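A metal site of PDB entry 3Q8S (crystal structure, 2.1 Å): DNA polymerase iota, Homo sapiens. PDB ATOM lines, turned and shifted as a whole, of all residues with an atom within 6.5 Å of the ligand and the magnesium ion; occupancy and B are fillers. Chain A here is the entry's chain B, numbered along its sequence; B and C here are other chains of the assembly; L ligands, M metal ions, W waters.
The side-chain amino group of Lys 214 is in salt-bridge range of an oxygen (O9) of the ligand (3.0 Å).
The backbone NH of Tyr 39 lies within hydrogen-bond range of an oxygen (O12) of the ligand (3.3 Å).
OH of Tyr 68 is in hydrogen-bond range of O7 of the ligand.
O9 of the ligand is in salt-bridge range of NZ of Lys 77, 2.7 Å away.
The guanidinium group of Arg 71 is in salt-bridge range of an oxygen (O9) of the ligand (3.0 Å).
The backbone NH of Phe 38 sits close to an oxygen (O4) of the ligand (3.3 Å).
The backbone NH of Cys 37 lies within hydrogen-bond range of an oxygen (O7) of the ligand, at 3.0 Å.
The side-chain hydroxyl (OG1) of Thr 65 is in hydrogen-bond range of an oxygen (O5) of the ligand, 2.9 Å away.
N1 of DG 5 of chain B is in hydrogen-bond range of a nitrogen (N2) of the ligand, 3.5 Å away.
O8 of 8OG 4 of chain B is in hydrogen-bond range of N2 of the ligand, 2.8 Å away.
O2 of DC 7 of chain C sits close to N2 of DG 5 of chain B (2.7 Å).
NE of Arg 71 lies within hydrogen-bond range of O of Cys 66 (3.1 Å).
The side-chain hydroxyl (OH) of Tyr 68 lies within hydrogen-bond range of the guanidinium group (NH1) of Arg 71 (3.4 Å).
NH2 of Arg 71 lies within hydrogen-bond range of OG1 of Thr 65, at 3.4 Å.
The backbone NH of Leu 78 sits at hydrogen-bond distance from the backbone carbonyl oxygen of Val 64.
O8 of 8OG 4 of chain B sits close to OE1 of Gln 59 (3.1 Å).
Merely in contact with the ligand: DC 7 of chain C (3.3 Å), Glu 127 (3.6 Å), Asp 36 (3.7 Å) and Leu 78 (3.9 Å).
Hydrophobic or aromatic side chains within 4 Å of the ligand: Phe 38, Tyr 39, Tyr 68 and Leu 78.
Within 4 Å of the ligand: Asp 34, Leu 35, Asp 36, Cys 37, Phe 38, Tyr 39, Thr 65, Tyr 68, Arg 71, Lys 77, Leu 78, Asp 126, Glu 127, Lys 214, 8OG 4 of chain B, DG 5 of chain B and DC 7 of chain C.
The nearest printed residue that does not touch the ligand is Gln 59 (4.2 Å).
Of the 24 residues printed, 3 come within 4 Å of the magnesium ion.
O of Leu 35 binds the magnesium ion, 2.2 Å away.
The magnesium ion is bound by an oxygen (O4) of the ligand, 2.2 Å away.
The magnesium ion is bound by O8 of the ligand (2.2 Å).
The magnesium ion is bound by OD1 of Asp 34 (2.2 Å).
OD1 of Asp 126 is bound to the magnesium ion (2.3 Å).
Slightly farther from the magnesium ion lies O2 of the ligand (2.8 Å).
Water W4 lies within hydrogen-bond range of OH of Tyr 39 (2.6 Å), O13 of the ligand (2.6 Å), N3 of DG 5 of chain B (2.9 Å) and NE2 of Gln 59 (3.2 Å).
Water W6 lies within hydrogen-bond range of the side-chain carboxylate (OD1) of Asp 36 (2.6 Å), an oxygen (O7) of the ligand (2.7 Å) and the side-chain hydroxyl (OH) of Tyr 68 (2.8 Å).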
ATOM      1  N   ASP A  34     -23.509  -8.642 -33.047  1.00  0.00           N
ATOM      2  CA  ASP A  34     -24.294  -9.713 -32.452  1.00  0.00           C
ATOM      3  C   ASP A  34     -23.362 -10.589 -31.618  1.00  0.00           C
ATOM      4  O   ASP A  34     -22.508 -11.281 -32.158  1.00  0.00           O
ATOM      5  CB  ASP A  34     -24.934 -10.555 -33.573  1.00  0.00           C
ATOM      6  CG  ASP A  34     -25.979 -11.518 -33.043  1.00  0.00           C
ATOM      7  OD1 ASP A  34     -25.922 -11.839 -31.843  1.00  0.00           O
ATOM      8  OD2 ASP A  34     -26.857 -11.953 -33.809  1.00  0.00           O
ATOM      9  N   LEU A  35     -23.530 -10.542 -30.294  1.00  0.00           N
ATOM     10  CA  LEU A  35     -22.589 -11.222 -29.394  1.00  0.00           C
ATOM     11  C   LEU A  35     -22.735 -12.722 -29.469  1.00  0.00           C
ATOM     12  O   LEU A  35     -23.818 -13.225 -29.664  1.00  0.00           O
ATOM     13  CB  LEU A  35     -22.829 -10.768 -27.947  1.00  0.00           C
ATOM     14  CG  LEU A  35     -22.079  -9.532 -27.485  1.00  0.00           C
ATOM     15  CD1 LEU A  35     -21.970  -8.530 -28.586  1.00  0.00           C
ATOM     16  CD2 LEU A  35     -22.725  -8.893 -26.248  1.00  0.00           C
ATOM     17  N   ASP A  36     -21.631 -13.440 -29.311  1.00  0.00           N
ATOM     18  CA  ASP A  36     -21.692 -14.888 -29.296  1.00  0.00           C
ATOM     19  C   ASP A  36     -22.128 -15.626 -28.034  1.00  0.00           C
ATOM     20  O   ASP A  36     -21.530 -15.449 -26.963  1.00  0.00           O
ATOM     21  CB  ASP A  36     -20.284 -15.486 -29.427  1.00  0.00           C
ATOM     22  CG  ASP A  36     -19.610 -15.111 -30.733  1.00  0.00           C
ATOM     23  OD1 ASP A  36     -20.301 -15.021 -31.784  1.00  0.00           O
ATOM     24  OD2 ASP A  36     -18.389 -14.920 -30.718  1.00  0.00           O
ATOM     25  N   CYS A  37     -23.179 -16.452 -28.170  1.00  0.00           N
ATOM     26  CA  CYS A  37     -23.930 -17.080 -27.091  1.00  0.00           C
ATOM     27  C   CYS A  37     -23.970 -16.215 -25.824  1.00  0.00           C
ATOM     28  O   CYS A  37     -23.478 -16.616 -24.780  1.00  0.00           O
ATOM     29  CB  CYS A  37     -23.331 -18.458 -26.790  1.00  0.00           C
ATOM     30  SG  CYS A  37     -21.556 -18.457 -26.486  1.00  0.00           S
ATOM     31  N   PHE A  38     -24.602 -15.054 -25.932  1.00  0.00           N
ATOM     32  CA  PHE A  38     -24.456 -13.984 -24.939  1.00  0.00           C
ATOM     33  C   PHE A  38     -24.462 -14.406 -23.452  1.00  0.00           C
ATOM     34  O   PHE A  38     -23.466 -14.226 -22.765  1.00  0.00           O
ATOM     35  CB  PHE A  38     -25.466 -12.861 -25.165  1.00  0.00           C
ATOM     36  CG  PHE A  38     -25.261 -11.683 -24.250  1.00  0.00           C
ATOM     37  CD1 PHE A  38     -24.003 -11.137 -24.085  1.00  0.00           C
ATOM     38  CD2 PHE A  38     -26.322 -11.132 -23.563  1.00  0.00           C
ATOM     39  CE1 PHE A  38     -23.801 -10.052 -23.233  1.00  0.00           C
ATOM     40  CE2 PHE A  38     -26.133 -10.052 -22.721  1.00  0.00           C
ATOM     41  CZ  PHE A  38     -24.876  -9.506 -22.565  1.00  0.00           C
ATOM     42  N   TYR A  39     -25.583 -14.935 -22.967  1.00  0.00           N
ATOM     43  CA  TYR A  39     -25.680 -15.280 -21.536  1.00  0.00           C
ATOM     44  C   TYR A  39     -24.562 -16.234 -21.126  1.00  0.00           C
ATOM     45  O   TYR A  39     -23.887 -16.019 -20.125  1.00  0.00           O
ATOM     46  CB  TYR A  39     -27.028 -15.925 -21.203  1.00  0.00           C
ATOM     47  CG  TYR A  39     -28.213 -14.998 -21.254  1.00  0.00           C
ATOM     48  CD1 TYR A  39     -29.476 -15.471 -20.916  1.00  0.00           C
ATOM     49  CD2 TYR A  39     -28.099 -13.675 -21.674  1.00  0.00           C
ATOM     50  CE1 TYR A  39     -30.588 -14.636 -20.960  1.00  0.00           C
ATOM     51  CE2 TYR A  39     -29.207 -12.831 -21.727  1.00  0.00           C
ATOM     52  CZ  TYR A  39     -30.449 -13.333 -21.371  1.00  0.00           C
ATOM     53  OH  TYR A  39     -31.562 -12.530 -21.416  1.00  0.00           O
ATOM     54  N   ALA A  40     -24.376 -17.282 -21.921  1.00  0.00           N
ATOM     55  CA  ALA A  40     -23.349 -18.274 -21.651  1.00  0.00           C
ATOM     56  C   ALA A  40     -21.959 -17.624 -21.594  1.00  0.00           C
ATOM     57  O   ALA A  40     -21.151 -17.965 -20.742  1.00  0.00           O
ATOM     58  CB  ALA A  40     -23.373 -19.387 -22.686  1.00  0.00           C
ATOM     59  N   GLN A  59     -33.430 -21.370 -17.550  1.00  0.00           N
ATOM     60  CA  GLN A  59     -34.486 -20.562 -16.975  1.00  0.00           C
ATOM     61  C   GLN A  59     -35.706 -21.461 -16.802  1.00  0.00           C
ATOM     62  O   GLN A  59     -36.326 -21.879 -17.769  1.00  0.00           O
ATOM     63  CB  GLN A  59     -34.802 -19.366 -17.886  1.00  0.00           C
ATOM     64  CG  GLN A  59     -33.732 -18.277 -17.882  1.00  0.00           C
ATOM     65  CD  GLN A  59     -34.032 -17.149 -18.865  1.00  0.00           C
ATOM     66  OE1 GLN A  59     -34.781 -17.339 -19.814  1.00  0.00           O
ATOM     67  NE2 GLN A  59     -33.447 -15.975 -18.624  1.00  0.00           N
ATOM     68  N   VAL A  64     -32.168 -21.636 -22.363  1.00  0.00           N
ATOM     69  CA  VAL A  64     -32.382 -20.510 -23.257  1.00  0.00           C
ATOM     70  C   VAL A  64     -31.255 -20.373 -24.273  1.00  0.00           C
ATOM     71  O   VAL A  64     -31.498 -20.039 -25.431  1.00  0.00           O
ATOM     72  CB  VAL A  64     -32.616 -19.188 -22.493  1.00  0.00           C
ATOM     73  CG1 VAL A  64     -33.760 -19.370 -21.537  1.00  0.00           C
ATOM     74  CG2 VAL A  64     -31.362 -18.742 -21.741  1.00  0.00           C
ATOM     75  N   THR A  65     -30.034 -20.641 -23.843  1.00  0.00           N
ATOM     76  CA  THR A  65     -28.892 -20.641 -24.744  1.00  0.00           C
ATOM     77  C   THR A  65     -27.757 -21.500 -24.171  1.00  0.00           C
ATOM     78  O   THR A  65     -27.784 -21.873 -23.002  1.00  0.00           O
ATOM     79  CB  THR A  65     -28.372 -19.205 -25.025  1.00  0.00           C
ATOM     80  OG1 THR A  65     -27.495 -19.218 -26.154  1.00  0.00           O
ATOM     81  CG2 THR A  65     -27.643 -18.621 -23.823  1.00  0.00           C
ATOM     82  N   CYS A  66     -26.778 -21.804 -25.010  1.00  0.00           N
ATOM     83  CA  CYS A  66     -25.630 -22.619 -24.616  1.00  0.00           C
ATOM     84  C   CYS A  66     -24.397 -22.176 -25.394  1.00  0.00           C
ATOM     85  O   CYS A  66     -24.524 -21.588 -26.465  1.00  0.00           O
ATOM     86  CB  CYS A  66     -25.920 -24.092 -24.899  1.00  0.00           C
ATOM     87  SG  CYS A  66     -26.353 -24.451 -26.627  1.00  0.00           S
ATOM     88  N   TYR A  68     -20.716 -22.763 -27.548  1.00  0.00           N
ATOM     89  CA  TYR A  68     -20.501 -23.501 -28.793  1.00  0.00           C
ATOM     90  C   TYR A  68     -19.942 -24.894 -28.582  1.00  0.00           C
ATOM     91  O   TYR A  68     -20.065 -25.763 -29.448  1.00  0.00           O
ATOM     92  CB  TYR A  68     -19.664 -22.672 -29.776  1.00  0.00           C
ATOM     93  CG  TYR A  68     -20.507 -21.620 -30.446  1.00  0.00           C
ATOM     94  CD1 TYR A  68     -20.778 -20.419 -29.816  1.00  0.00           C
ATOM     95  CD2 TYR A  68     -21.061 -21.840 -31.708  1.00  0.00           C
ATOM     96  CE1 TYR A  68     -21.566 -19.453 -30.409  1.00  0.00           C
ATOM     97  CE2 TYR A  68     -21.852 -20.883 -32.321  1.00  0.00           C
ATOM     98  CZ  TYR A  68     -22.092 -19.684 -31.672  1.00  0.00           C
ATOM     99  OH  TYR A  68     -22.879 -18.718 -32.255  1.00  0.00           O
ATOM    100  N   ARG A  71     -23.256 -26.741 -28.418  1.00  0.00           N
ATOM    101  CA  ARG A  71     -23.963 -26.884 -29.686  1.00  0.00           C
ATOM    102  C   ARG A  71     -23.307 -27.953 -30.536  1.00  0.00           C
ATOM    103  O   ARG A  71     -23.961 -28.618 -31.341  1.00  0.00           O
ATOM    104  CB  ARG A  71     -24.020 -25.542 -30.435  1.00  0.00           C
ATOM    105  CG  ARG A  71     -24.672 -24.431 -29.624  1.00  0.00           C
ATOM    106  CD  ARG A  71     -24.745 -23.104 -30.372  1.00  0.00           C
ATOM    107  NE  ARG A  71     -25.083 -22.014 -29.465  1.00  0.00           N
ATOM    108  CZ  ARG A  71     -25.440 -20.786 -29.854  1.00  0.00           C
ATOM    109  NH1 ARG A  71     -25.505 -20.482 -31.144  1.00  0.00           N
ATOM    110  NH2 ARG A  71     -25.723 -19.866 -28.942  1.00  0.00           N
ATOM    111  N   LYS A  77     -30.577 -23.871 -28.951  1.00  0.00           N
ATOM    112  CA  LYS A  77     -31.179 -22.765 -28.200  1.00  0.00           C
ATOM    113  C   LYS A  77     -32.628 -23.075 -27.846  1.00  0.00           C
ATOM    114  O   LYS A  77     -33.376 -23.620 -28.646  1.00  0.00           O
ATOM    115  CB  LYS A  77     -31.124 -21.463 -29.001  1.00  0.00           C
ATOM    116  CG  LYS A  77     -29.721 -20.988 -29.329  1.00  0.00           C
ATOM    117  CD  LYS A  77     -29.772 -19.579 -29.926  1.00  0.00           C
ATOM    118  CE  LYS A  77     -28.985 -19.480 -31.231  1.00  0.00           C
ATOM    119  NZ  LYS A  77     -29.122 -18.134 -31.848  1.00  0.00           N
ATOM    120  N   LEU A  78     -33.022 -22.708 -26.620  1.00  0.00           N
ATOM    121  CA  LEU A  78     -34.407 -22.851 -26.182  1.00  0.00           C
ATOM    122  C   LEU A  78     -34.876 -24.312 -26.103  1.00  0.00           C
ATOM    123  O   LEU A  78     -36.075 -24.582 -26.230  1.00  0.00           O
ATOM    124  CB  LEU A  78     -35.349 -22.055 -27.089  1.00  0.00           C
ATOM    125  CG  LEU A  78     -35.078 -20.552 -27.215  1.00  0.00           C
ATOM    126  CD1 LEU A  78     -35.711 -19.998 -28.482  1.00  0.00           C
ATOM    127  CD2 LEU A  78     -35.578 -19.806 -25.996  1.00  0.00           C
ATOM    128  N   LEU A  99     -31.542 -11.520 -14.651  1.00  0.00           N
ATOM    129  CA  LEU A  99     -30.888 -10.949 -15.820  1.00  0.00           C
ATOM    130  C   LEU A  99     -29.900  -9.840 -15.475  1.00  0.00           C
ATOM    131  O   LEU A  99     -29.331  -9.225 -16.382  1.00  0.00           O
ATOM    132  CB  LEU A  99     -31.922 -10.373 -16.783  1.00  0.00           C
ATOM    133  CG  LEU A  99     -32.999 -11.305 -17.352  1.00  0.00           C
ATOM    134  CD1 LEU A  99     -33.694 -10.634 -18.536  1.00  0.00           C
ATOM    135  CD2 LEU A  99     -32.397 -12.633 -17.759  1.00  0.00           C
ATOM    136  N   PHE A 125     -30.856  -7.768 -25.727  1.00  0.00           N
ATOM    137  CA  PHE A 125     -29.704  -7.522 -24.870  1.00  0.00           C
ATOM    138  C   PHE A 125     -28.364  -7.664 -25.557  1.00  0.00           C
ATOM    139  O   PHE A 125     -27.351  -7.165 -25.051  1.00  0.00           O
ATOM    140  CB  PHE A 125     -29.730  -8.420 -23.627  1.00  0.00           C
ATOM    141  CG  PHE A 125     -30.596  -7.910 -22.512  1.00  0.00           C
ATOM    142  CD1 PHE A 125     -31.430  -6.832 -22.701  1.00  0.00           C
ATOM    143  CD2 PHE A 125     -30.566  -8.510 -21.251  1.00  0.00           C
ATOM    144  CE1 PHE A 125     -32.237  -6.361 -21.678  1.00  0.00           C
ATOM    145  CE2 PHE A 125     -31.355  -8.046 -20.228  1.00  0.00           C
ATOM    146  CZ  PHE A 125     -32.189  -6.967 -20.437  1.00  0.00           C
ATOM    147  N   ASP A 126     -28.320  -8.352 -26.690  1.00  0.00           N
ATOM    148  CA  ASP A 126     -27.006  -8.659 -27.242  1.00  0.00           C
ATOM    149  C   ASP A 126     -26.758  -8.220 -28.691  1.00  0.00           C
ATOM    150  O   ASP A 126     -25.747  -8.596 -29.283  1.00  0.00           O
ATOM    151  CB  ASP A 126     -26.693 -10.142 -27.080  1.00  0.00           C
ATOM    152  CG  ASP A 126     -27.015 -10.949 -28.323  1.00  0.00           C
ATOM    153  OD1 ASP A 126     -26.127 -11.699 -28.765  1.00  0.00           O
ATOM    154  OD2 ASP A 126     -28.139 -10.820 -28.849  1.00  0.00           O
ATOM    155  N   GLU A 127     -27.645  -7.411 -29.248  1.00  0.00           N
ATOM    156  CA  GLU A 127     -27.448  -6.912 -30.615  1.00  0.00           C
ATOM    157  C   GLU A 127     -27.521  -5.392 -30.677  1.00  0.00           C
ATOM    158  O   GLU A 127     -28.296  -4.787 -29.951  1.00  0.00           O
ATOM    159  CB  GLU A 127     -28.469  -7.523 -31.575  1.00  0.00           C
ATOM    160  CG  GLU A 127     -28.249  -9.004 -31.823  1.00  0.00           C
ATOM    161  CD  GLU A 127     -29.396  -9.650 -32.563  1.00  0.00           C
ATOM    162  OE1 GLU A 127     -29.962  -8.991 -33.477  1.00  0.00           O
ATOM    163  OE2 GLU A 127     -29.737 -10.801 -32.245  1.00  0.00           O
ATOM    164  N   LYS A 214     -20.191 -17.761 -38.193  1.00  0.00           N
ATOM    165  CA  LYS A 214     -20.239 -17.741 -36.732  1.00  0.00           C
ATOM    166  C   LYS A 214     -19.429 -18.905 -36.195  1.00  0.00           C
ATOM    167  O   LYS A 214     -19.279 -19.911 -36.878  1.00  0.00           O
ATOM    168  CB  LYS A 214     -21.679 -17.919 -36.243  1.00  0.00           C
ATOM    169  CG  LYS A 214     -22.526 -16.679 -36.317  1.00  0.00           C
ATOM    170  CD  LYS A 214     -24.010 -17.042 -36.254  1.00  0.00           C
ATOM    171  CE  LYS A 214     -24.303 -17.938 -35.059  1.00  0.00           C
ATOM    172  NZ  LYS A 214     -25.766 -18.080 -34.799  1.00  0.00           N
ATOM    173  N   PRO A 215     -18.913 -18.788 -34.955  1.00  0.00           N
ATOM    174  CA  PRO A 215     -19.012 -17.592 -34.107  1.00  0.00           C
ATOM    175  C   PRO A 215     -17.803 -16.667 -34.290  1.00  0.00           C
ATOM    176  O   PRO A 215     -16.865 -17.002 -35.009  1.00  0.00           O
ATOM    177  CB  PRO A 215     -19.002 -18.168 -32.694  1.00  0.00           C
ATOM    178  CG  PRO A 215     -18.149 -19.383 -32.800  1.00  0.00           C
ATOM    179  CD  PRO A 215     -18.383 -19.941 -34.206  1.00  0.00           C
ATOM    180  P   8OG B   4     -42.845 -20.023 -19.211  1.00  0.00           P
ATOM    181  OP1 8OG B   4     -43.689 -20.586 -18.110  1.00  0.00           O
ATOM    182  OP2 8OG B   4     -42.801 -20.727 -20.554  1.00  0.00           O
ATOM    183  O5' 8OG B   4     -41.345 -19.885 -18.661  1.00  0.00           O
ATOM    184  C5' 8OG B   4     -40.247 -20.093 -19.548  1.00  0.00           C
ATOM    185  C4' 8OG B   4     -39.020 -19.298 -19.105  1.00  0.00           C
ATOM    186  O4' 8OG B   4     -38.230 -19.024 -20.254  1.00  0.00           O
ATOM    187  C3' 8OG B   4     -39.360 -17.966 -18.440  1.00  0.00           C
ATOM    188  O3' 8OG B   4     -38.534 -17.843 -17.273  1.00  0.00           O
ATOM    189  C2' 8OG B   4     -38.973 -16.908 -19.471  1.00  0.00           C
ATOM    190  C1' 8OG B   4     -38.083 -17.622 -20.482  1.00  0.00           C
ATOM    191  N9  8OG B   4     -38.338 -17.276 -21.910  1.00  0.00           N
ATOM    192  C8  8OG B   4     -37.425 -16.914 -22.818  1.00  0.00           C
ATOM    193  N7  8OG B   4     -37.854 -16.649 -24.046  1.00  0.00           N
ATOM    194  C5  8OG B   4     -39.170 -16.872 -23.961  1.00  0.00           C
ATOM    195  C6  8OG B   4     -40.287 -16.787 -24.928  1.00  0.00           C
ATOM    196  O6  8OG B   4     -40.058 -16.444 -26.100  1.00  0.00           O
ATOM    197  N1  8OG B   4     -41.516 -17.083 -24.495  1.00  0.00           N
ATOM    198  C2  8OG B   4     -41.764 -17.454 -23.224  1.00  0.00           C
ATOM    199  N2  8OG B   4     -43.047 -17.749 -22.881  1.00  0.00           N
ATOM    200  N3  8OG B   4     -40.792 -17.559 -22.286  1.00  0.00           N
ATOM    201  C4  8OG B   4     -39.493 -17.281 -22.580  1.00  0.00           C
ATOM    202  O8  8OG B   4     -36.213 -16.791 -22.535  1.00  0.00           O
ATOM    203  P    DG B   5     -38.818 -16.824 -16.068  1.00  0.00           P
ATOM    204  OP1  DG B   5     -38.044 -17.163 -14.855  1.00  0.00           O
ATOM    205  OP2  DG B   5     -40.270 -16.602 -16.028  1.00  0.00           O
ATOM    206  O5'  DG B   5     -38.103 -15.536 -16.665  1.00  0.00           O
ATOM    207  C5'  DG B   5     -36.708 -15.285 -16.491  1.00  0.00           C
ATOM    208  C4'  DG B   5     -36.344 -13.962 -17.143  1.00  0.00           C
ATOM    209  O4'  DG B   5     -36.592 -14.066 -18.565  1.00  0.00           O
ATOM    210  C3'  DG B   5     -37.203 -12.786 -16.679  1.00  0.00           C
ATOM    211  O3'  DG B   5     -36.440 -11.607 -16.649  1.00  0.00           O
ATOM    212  C2'  DG B   5     -38.274 -12.684 -17.746  1.00  0.00           C
ATOM    213  C1'  DG B   5     -37.367 -12.962 -18.944  1.00  0.00           C
ATOM    214  N9   DG B   5     -38.072 -13.245 -20.176  1.00  0.00           N
ATOM    215  C8   DG B   5     -39.326 -13.781 -20.351  1.00  0.00           C
ATOM    216  N7   DG B   5     -39.668 -13.888 -21.612  1.00  0.00           N
ATOM    217  C5   DG B   5     -38.557 -13.403 -22.298  1.00  0.00           C
ATOM    218  C6   DG B   5     -38.336 -13.275 -23.687  1.00  0.00           C
ATOM    219  O6   DG B   5     -39.095 -13.578 -24.619  1.00  0.00           O
ATOM    220  N1   DG B   5     -37.086 -12.725 -23.942  1.00  0.00           N
ATOM    221  C2   DG B   5     -36.164 -12.354 -22.998  1.00  0.00           C
ATOM    222  N2   DG B   5     -35.005 -11.839 -23.463  1.00  0.00           N
ATOM    223  N3   DG B   5     -36.353 -12.480 -21.700  1.00  0.00           N
ATOM    224  C4   DG B   5     -37.571 -12.999 -21.434  1.00  0.00           C
ATOM    225  P    DC C   7     -34.725 -11.744 -33.728  1.00  0.00           P
ATOM    226  OP1  DC C   7     -33.686 -11.991 -34.736  1.00  0.00           O
ATOM    227  OP2  DC C   7     -35.911 -12.634 -33.585  1.00  0.00           O
ATOM    228  O5'  DC C   7     -34.035 -11.718 -32.263  1.00  0.00           O
ATOM    229  C5'  DC C   7     -32.977 -10.792 -32.004  1.00  0.00           C
ATOM    230  C4'  DC C   7     -32.586 -10.826 -30.538  1.00  0.00           C
ATOM    231  O4'  DC C   7     -33.643 -10.237 -29.730  1.00  0.00           O
ATOM    232  C3'  DC C   7     -32.399 -12.211 -29.933  1.00  0.00           C
ATOM    233  C2'  DC C   7     -32.561 -11.895 -28.441  1.00  0.00           C
ATOM    234  C1'  DC C   7     -33.690 -10.872 -28.478  1.00  0.00           C
ATOM    235  N1   DC C   7     -35.025 -11.507 -28.275  1.00  0.00           N
ATOM    236  C2   DC C   7     -35.405 -11.745 -26.958  1.00  0.00           C
ATOM    237  O2   DC C   7     -34.623 -11.406 -26.065  1.00  0.00           O
ATOM    238  N3   DC C   7     -36.603 -12.325 -26.715  1.00  0.00           N
ATOM    239  C4   DC C   7     -37.382 -12.650 -27.748  1.00  0.00           C
ATOM    240  N4   DC C   7     -38.558 -13.228 -27.475  1.00  0.00           N
ATOM    241  C5   DC C   7     -37.007 -12.420 -29.096  1.00  0.00           C
ATOM    242  C6   DC C   7     -35.821 -11.847 -29.319  1.00  0.00           C
HETATM  243  P1  LIG L   1     -29.494 -14.649 -29.635  1.00  0.00           P
HETATM  244  O1  LIG L   1     -30.673 -14.938 -30.524  1.00  0.00           O
HETATM  245  O2  LIG L   1     -28.691 -13.501 -30.167  1.00  0.00           O
HETATM  246  O3  LIG L   1     -28.575 -15.960 -29.484  1.00  0.00           O
HETATM  247  P2  LIG L   1     -27.205 -16.017 -28.639  1.00  0.00           P
HETATM  248  O4  LIG L   1     -26.532 -14.679 -28.533  1.00  0.00           O
HETATM  249  O5  LIG L   1     -27.492 -16.588 -27.273  1.00  0.00           O
HETATM  250  O6  LIG L   1     -26.295 -17.064 -29.440  1.00  0.00           O
HETATM  251  P3  LIG L   1     -25.719 -16.776 -30.917  1.00  0.00           P
HETATM  252  O7  LIG L   1     -24.247 -17.060 -30.910  1.00  0.00           O
HETATM  253  O8  LIG L   1     -25.963 -15.354 -31.331  1.00  0.00           O
HETATM  254  O9  LIG L   1     -26.411 -17.711 -31.860  1.00  0.00           O
HETATM  255  O10 LIG L   1     -30.007 -14.332 -28.140  1.00  0.00           O
HETATM  256  C1  LIG L   1     -29.341 -13.373 -27.326  1.00  0.00           C
HETATM  257  C2  LIG L   1     -29.657 -13.649 -25.861  1.00  0.00           C
HETATM  258  O11 LIG L   1     -31.027 -13.335 -25.578  1.00  0.00           O
HETATM  259  C3  LIG L   1     -29.462 -15.115 -25.528  1.00  0.00           C
HETATM  260  O12 LIG L   1     -28.245 -15.294 -24.804  1.00  0.00           O
HETATM  261  C4  LIG L   1     -30.655 -15.510 -24.688  1.00  0.00           C
HETATM  262  C5  LIG L   1     -31.611 -14.338 -24.743  1.00  0.00           C
HETATM  263  N1  LIG L   1     -32.905 -14.786 -25.265  1.00  0.00           N
HETATM  264  C6  LIG L   1     -33.961 -15.074 -24.374  1.00  0.00           C
HETATM  265  O13 LIG L   1     -33.767 -14.934 -23.141  1.00  0.00           O
HETATM  266  N2  LIG L   1     -35.158 -15.496 -24.806  1.00  0.00           N
HETATM  267  C7  LIG L   1     -35.381 -15.655 -26.109  1.00  0.00           C
HETATM  268  O14 LIG L   1     -36.492 -16.047 -26.521  1.00  0.00           O
HETATM  269  C8  LIG L   1     -34.300 -15.354 -27.071  1.00  0.00           C
HETATM  270  C9  LIG L   1     -34.545 -15.533 -28.545  1.00  0.00           C
HETATM  271  C10 LIG L   1     -33.077 -14.921 -26.589  1.00  0.00           C
HETATM  272 MG    MG M   1     -25.939 -13.401 -30.230  1.00  0.00          MG
HETATM  273  O   HOH W   1     -24.053 -13.476 -32.481  1.00  0.00           O
HETATM  274  O   HOH W   2     -31.562 -14.441 -32.871  1.00  0.00           O
HETATM  275  O   HOH W   3     -37.329 -16.291 -29.703  1.00  0.00           O
HETATM  276  O   HOH W   4     -33.867 -13.650 -20.829  1.00  0.00           O
HETATM  277  O   HOH W   5     -27.767 -14.684 -33.555  1.00  0.00           O
HETATM  278  O   HOH W   6     -22.511 -15.942 -32.712  1.00  0.00           O
